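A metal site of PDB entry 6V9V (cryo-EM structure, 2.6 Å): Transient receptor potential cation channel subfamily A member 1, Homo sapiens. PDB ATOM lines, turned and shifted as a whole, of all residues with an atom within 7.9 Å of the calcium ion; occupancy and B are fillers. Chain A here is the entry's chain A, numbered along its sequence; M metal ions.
The calcium ion is bound by the side-chain amide oxygen (OE1) of Gln 791 (2.5 Å), the side-chain carboxylate (OE1) of Glu 808 (2.5 Å), the side-chain amide oxygen (OD1) of Asn 805 (2.6 Å) and the side-chain carboxylate (OE2) of Glu 808 (2.7 Å). The calcium ion has four donor atoms within binding distance. Slightly farther from the calcium ion lies the side-chain carboxylate (OE2) of Glu 788 (3.1 Å). Slightly farther from the calcium ion lies NE2 of Gln 791 (3.1 Å).
Four residues have an atom within 4 Å of the calcium ion: Glu 788, Gln 791, Asn 805 and Glu 808.
The side-chain amide oxygen of Gln 791 sits close to the side-chain carboxylate of Glu 788 (3.0 Å). OD1 of Asn 805 lies close to OE1 of Glu 788 (3.5 Å). The backbone carbonyl oxygen (O) of Tyr 799 sits at hydrogen-bond distance from the side-chain amide nitrogen (ND2) of Asn 805, at 3.0 Å.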
ATOM      1  N   ASN A 722     -15.150   8.506  10.216  1.00  0.00           N
ATOM      2  CA  ASN A 722     -16.319   9.374  10.149  1.00  0.00           C
ATOM      3  C   ASN A 722     -16.768   9.792  11.536  1.00  0.00           C
ATOM      4  O   ASN A 722     -17.068  10.965  11.772  1.00  0.00           O
ATOM      5  CB  ASN A 722     -17.446   8.659   9.418  1.00  0.00           C
ATOM      6  CG  ASN A 722     -18.503   9.619   8.933  1.00  0.00           C
ATOM      7  OD1 ASN A 722     -18.314  10.829   8.957  1.00  0.00           O
ATOM      8  ND2 ASN A 722     -19.626   9.081   8.481  1.00  0.00           N
ATOM      9  N   GLY A 784     -15.353  19.651   8.159  1.00  0.00           N
ATOM     10  CA  GLY A 784     -16.728  19.332   7.832  1.00  0.00           C
ATOM     11  C   GLY A 784     -17.256  20.062   6.616  1.00  0.00           C
ATOM     12  O   GLY A 784     -18.218  19.598   6.001  1.00  0.00           O
ATOM     13  N   LYS A 787     -15.841  17.889   3.957  1.00  0.00           N
ATOM     14  CA  LYS A 787     -16.632  16.666   3.980  1.00  0.00           C
ATOM     15  C   LYS A 787     -17.991  16.901   3.326  1.00  0.00           C
ATOM     16  O   LYS A 787     -18.503  16.023   2.621  1.00  0.00           O
ATOM     17  CB  LYS A 787     -16.793  16.167   5.413  1.00  0.00           C
ATOM     18  CG  LYS A 787     -17.481  14.832   5.519  1.00  0.00           C
ATOM     19  CD  LYS A 787     -17.800  14.492   6.966  1.00  0.00           C
ATOM     20  CE  LYS A 787     -16.542  14.460   7.812  1.00  0.00           C
ATOM     21  NZ  LYS A 787     -16.855  14.159   9.226  1.00  0.00           N
ATOM     22  N   GLU A 788     -18.587  18.063   3.550  1.00  0.00           N
ATOM     23  CA  GLU A 788     -19.866  18.357   2.917  1.00  0.00           C
ATOM     24  C   GLU A 788     -19.694  18.770   1.460  1.00  0.00           C
ATOM     25  O   GLU A 788     -20.535  18.414   0.631  1.00  0.00           O
ATOM     26  CB  GLU A 788     -20.627  19.424   3.689  1.00  0.00           C
ATOM     27  CG  GLU A 788     -21.263  18.920   4.965  1.00  0.00           C
ATOM     28  CD  GLU A 788     -22.057  17.640   4.751  1.00  0.00           C
ATOM     29  OE1 GLU A 788     -23.079  17.686   4.044  1.00  0.00           O
ATOM     30  OE2 GLU A 788     -21.669  16.592   5.312  1.00  0.00           O
ATOM     31  N   GLN A 791     -19.388  15.838  -0.400  1.00  0.00           N
ATOM     32  CA  GLN A 791     -20.644  15.126  -0.535  1.00  0.00           C
ATOM     33  C   GLN A 791     -21.501  15.690  -1.658  1.00  0.00           C
ATOM     34  O   GLN A 791     -22.226  14.924  -2.309  1.00  0.00           O
ATOM     35  CB  GLN A 791     -21.411  15.168   0.783  1.00  0.00           C
ATOM     36  CG  GLN A 791     -21.050  14.056   1.740  1.00  0.00           C
ATOM     37  CD  GLN A 791     -21.843  14.106   3.022  1.00  0.00           C
ATOM     38  OE1 GLN A 791     -22.774  14.886   3.156  1.00  0.00           O
ATOM     39  NE2 GLN A 791     -21.466  13.267   3.989  1.00  0.00           N
ATOM     40  N   GLN A 795     -22.732  13.579  -4.769  1.00  0.00           N
ATOM     41  CA  GLN A 795     -24.192  13.557  -4.848  1.00  0.00           C
ATOM     42  C   GLN A 795     -24.636  14.938  -5.326  1.00  0.00           C
ATOM     43  O   GLN A 795     -24.681  15.892  -4.550  1.00  0.00           O
ATOM     44  CB  GLN A 795     -24.813  13.216  -3.505  1.00  0.00           C
ATOM     45  CG  GLN A 795     -24.115  12.116  -2.758  1.00  0.00           C
ATOM     46  CD  GLN A 795     -24.590  12.012  -1.326  1.00  0.00           C
ATOM     47  OE1 GLN A 795     -25.323  12.864  -0.841  1.00  0.00           O
ATOM     48  NE2 GLN A 795     -24.171  10.947  -0.637  1.00  0.00           N
ATOM     49  N   TYR A 799     -28.246  15.441  -2.998  1.00  0.00           N
ATOM     50  CA  TYR A 799     -27.793  15.949  -1.713  1.00  0.00           C
ATOM     51  C   TYR A 799     -28.860  16.794  -1.060  1.00  0.00           C
ATOM     52  O   TYR A 799     -29.127  16.669   0.138  1.00  0.00           O
ATOM     53  CB  TYR A 799     -26.516  16.773  -1.936  1.00  0.00           C
ATOM     54  CG  TYR A 799     -25.920  17.403  -0.709  1.00  0.00           C
ATOM     55  CD1 TYR A 799     -24.995  16.714   0.051  1.00  0.00           C
ATOM     56  CD2 TYR A 799     -26.233  18.701  -0.335  1.00  0.00           C
ATOM     57  CE1 TYR A 799     -24.420  17.287   1.160  1.00  0.00           C
ATOM     58  CE2 TYR A 799     -25.685  19.276   0.778  1.00  0.00           C
ATOM     59  CZ  TYR A 799     -24.773  18.569   1.516  1.00  0.00           C
ATOM     60  OH  TYR A 799     -24.211  19.142   2.626  1.00  0.00           O
ATOM     61  N   ASP A 802     -32.077  15.801   1.255  1.00  0.00           N
ATOM     62  CA  ASP A 802     -31.743  15.163   2.516  1.00  0.00           C
ATOM     63  C   ASP A 802     -31.815  16.230   3.595  1.00  0.00           C
ATOM     64  O   ASP A 802     -31.232  17.310   3.446  1.00  0.00           O
ATOM     65  CB  ASP A 802     -30.353  14.533   2.457  1.00  0.00           C
ATOM     66  CG  ASP A 802     -30.002  13.710   3.685  1.00  0.00           C
ATOM     67  OD1 ASP A 802     -30.793  13.621   4.654  1.00  0.00           O
ATOM     68  OD2 ASP A 802     -28.920  13.096   3.664  1.00  0.00           O
ATOM     69  N   SER A 804     -30.690  15.783   6.768  1.00  0.00           N
ATOM     70  CA  SER A 804     -29.556  15.717   7.670  1.00  0.00           C
ATOM     71  C   SER A 804     -28.411  16.626   7.226  1.00  0.00           C
ATOM     72  O   SER A 804     -27.565  16.978   8.043  1.00  0.00           O
ATOM     73  CB  SER A 804     -29.045  14.289   7.785  1.00  0.00           C
ATOM     74  OG  SER A 804     -28.625  13.818   6.521  1.00  0.00           O
ATOM     75  N   ASN A 805     -28.373  17.000   5.949  1.00  0.00           N
ATOM     76  CA  ASN A 805     -27.294  17.850   5.481  1.00  0.00           C
ATOM     77  C   ASN A 805     -27.456  19.278   5.948  1.00  0.00           C
ATOM     78  O   ASN A 805     -26.454  19.970   6.170  1.00  0.00           O
ATOM     79  CB  ASN A 805     -27.188  17.775   3.972  1.00  0.00           C
ATOM     80  CG  ASN A 805     -26.759  16.412   3.489  1.00  0.00           C
ATOM     81  OD1 ASN A 805     -25.977  15.740   4.148  1.00  0.00           O
ATOM     82  ND2 ASN A 805     -27.284  16.001   2.343  1.00  0.00           N
ATOM     83  N   VAL A 806     -28.690  19.753   6.134  1.00  0.00           N
ATOM     84  CA  VAL A 806     -28.840  21.122   6.607  1.00  0.00           C
ATOM     85  C   VAL A 806     -28.541  21.201   8.095  1.00  0.00           C
ATOM     86  O   VAL A 806     -28.194  22.273   8.597  1.00  0.00           O
ATOM     87  CB  VAL A 806     -30.243  21.680   6.272  1.00  0.00           C
ATOM     88  CG1 VAL A 806     -31.319  21.125   7.197  1.00  0.00           C
ATOM     89  CG2 VAL A 806     -30.250  23.195   6.268  1.00  0.00           C
ATOM     90  N   GLU A 808     -25.959  19.628   9.344  1.00  0.00           N
ATOM     91  CA  GLU A 808     -24.507  19.773   9.351  1.00  0.00           C
ATOM     92  C   GLU A 808     -24.092  21.185   9.001  1.00  0.00           C
ATOM     93  O   GLU A 808     -23.114  21.697   9.553  1.00  0.00           O
ATOM     94  CB  GLU A 808     -23.899  18.778   8.377  1.00  0.00           C
ATOM     95  CG  GLU A 808     -23.954  17.346   8.845  1.00  0.00           C
ATOM     96  CD  GLU A 808     -23.929  16.352   7.701  1.00  0.00           C
ATOM     97  OE1 GLU A 808     -24.355  16.723   6.587  1.00  0.00           O
ATOM     98  OE2 GLU A 808     -23.470  15.211   7.907  1.00  0.00           O
ATOM     99  N   TRP A 809     -24.842  21.846   8.121  1.00  0.00           N
ATOM    100  CA  TRP A 809     -24.472  23.202   7.738  1.00  0.00           C
ATOM    101  C   TRP A 809     -24.701  24.190   8.858  1.00  0.00           C
ATOM    102  O   TRP A 809     -23.972  25.169   8.979  1.00  0.00           O
ATOM    103  CB  TRP A 809     -25.231  23.609   6.480  1.00  0.00           C
ATOM    104  CG  TRP A 809     -24.571  23.137   5.242  1.00  0.00           C
ATOM    105  CD1 TRP A 809     -24.932  22.076   4.486  1.00  0.00           C
ATOM    106  CD2 TRP A 809     -23.421  23.710   4.618  1.00  0.00           C
ATOM    107  NE1 TRP A 809     -24.078  21.948   3.418  1.00  0.00           N
ATOM    108  CE2 TRP A 809     -23.142  22.937   3.476  1.00  0.00           C
ATOM    109  CE3 TRP A 809     -22.594  24.790   4.913  1.00  0.00           C
ATOM    110  CZ2 TRP A 809     -22.083  23.214   2.629  1.00  0.00           C
ATOM    111  CZ3 TRP A 809     -21.541  25.064   4.072  1.00  0.00           C
ATOM    112  CH2 TRP A 809     -21.290  24.284   2.946  1.00  0.00           C
ATOM    113  N   TYR A 812     -21.575  23.532  11.312  1.00  0.00           N
ATOM    114  CA  TYR A 812     -20.196  23.916  11.035  1.00  0.00           C
ATOM    115  C   TYR A 812     -20.025  25.420  11.035  1.00  0.00           C
ATOM    116  O   TYR A 812     -18.958  25.900  11.426  1.00  0.00           O
ATOM    117  CB  TYR A 812     -19.722  23.303   9.726  1.00  0.00           C
ATOM    118  CG  TYR A 812     -19.641  21.808   9.785  1.00  0.00           C
ATOM    119  CD1 TYR A 812     -19.013  21.169  10.847  1.00  0.00           C
ATOM    120  CD2 TYR A 812     -20.201  21.023   8.794  1.00  0.00           C
ATOM    121  CE1 TYR A 812     -18.950  19.797  10.917  1.00  0.00           C
ATOM    122  CE2 TYR A 812     -20.153  19.645   8.860  1.00  0.00           C
ATOM    123  CZ  TYR A 812     -19.523  19.046   9.919  1.00  0.00           C
ATOM    124  OH  TYR A 812     -19.468  17.672   9.978  1.00  0.00           O
ATOM    125  N   ASN A 845     -27.055  15.710  16.236  1.00  0.00           N
ATOM    126  CA  ASN A 845     -26.575  15.062  15.034  1.00  0.00           C
ATOM    127  C   ASN A 845     -25.741  13.839  15.351  1.00  0.00           C
ATOM    128  O   ASN A 845     -25.669  12.917  14.545  1.00  0.00           O
ATOM    129  CB  ASN A 845     -25.768  16.045  14.204  1.00  0.00           C
ATOM    130  CG  ASN A 845     -25.370  15.502  12.874  1.00  0.00           C
ATOM    131  OD1 ASN A 845     -26.168  14.888  12.180  1.00  0.00           O
ATOM    132  ND2 ASN A 845     -24.118  15.712  12.504  1.00  0.00           N
ATOM    133  N   TYR A 849     -25.346   9.583  14.017  1.00  0.00           N
ATOM    134  CA  TYR A 849     -24.182   8.791  13.662  1.00  0.00           C
ATOM    135  C   TYR A 849     -24.180   7.418  14.302  1.00  0.00           C
ATOM    136  O   TYR A 849     -23.387   6.562  13.890  1.00  0.00           O
ATOM    137  CB  TYR A 849     -22.898   9.533  14.030  1.00  0.00           C
ATOM    138  CG  TYR A 849     -22.487  10.559  13.012  1.00  0.00           C
ATOM    139  CD1 TYR A 849     -23.215  10.733  11.845  1.00  0.00           C
ATOM    140  CD2 TYR A 849     -21.368  11.341  13.206  1.00  0.00           C
ATOM    141  CE1 TYR A 849     -22.842  11.668  10.903  1.00  0.00           C
ATOM    142  CE2 TYR A 849     -20.994  12.284  12.270  1.00  0.00           C
ATOM    143  CZ  TYR A 849     -21.734  12.441  11.128  1.00  0.00           C
ATOM    144  OH  TYR A 849     -21.353  13.379  10.196  1.00  0.00           O
ATOM    145  N   ARG A 852     -26.013   4.047  12.353  1.00  0.00           N
ATOM    146  CA  ARG A 852     -25.198   3.031  11.682  1.00  0.00           C
ATOM    147  C   ARG A 852     -24.545   2.089  12.680  1.00  0.00           C
ATOM    148  O   ARG A 852     -23.339   1.853  12.672  1.00  0.00           O
ATOM    149  CB  ARG A 852     -24.160   3.734  10.808  1.00  0.00           C
ATOM    150  CG  ARG A 852     -24.729   4.283   9.503  1.00  0.00           C
ATOM    151  CD  ARG A 852     -25.176   5.726   9.614  1.00  0.00           C
ATOM    152  NE  ARG A 852     -24.056   6.629   9.851  1.00  0.00           N
ATOM    153  CZ  ARG A 852     -23.453   7.319   8.902  1.00  0.00           C
ATOM    154  NH1 ARG A 852     -22.446   8.129   9.201  1.00  0.00           N
ATOM    155  NH2 ARG A 852     -23.864   7.221   7.644  1.00  0.00           N
HETATM  156 CA    CA M   1     -23.966  14.559   5.351  1.00  0.00          CA
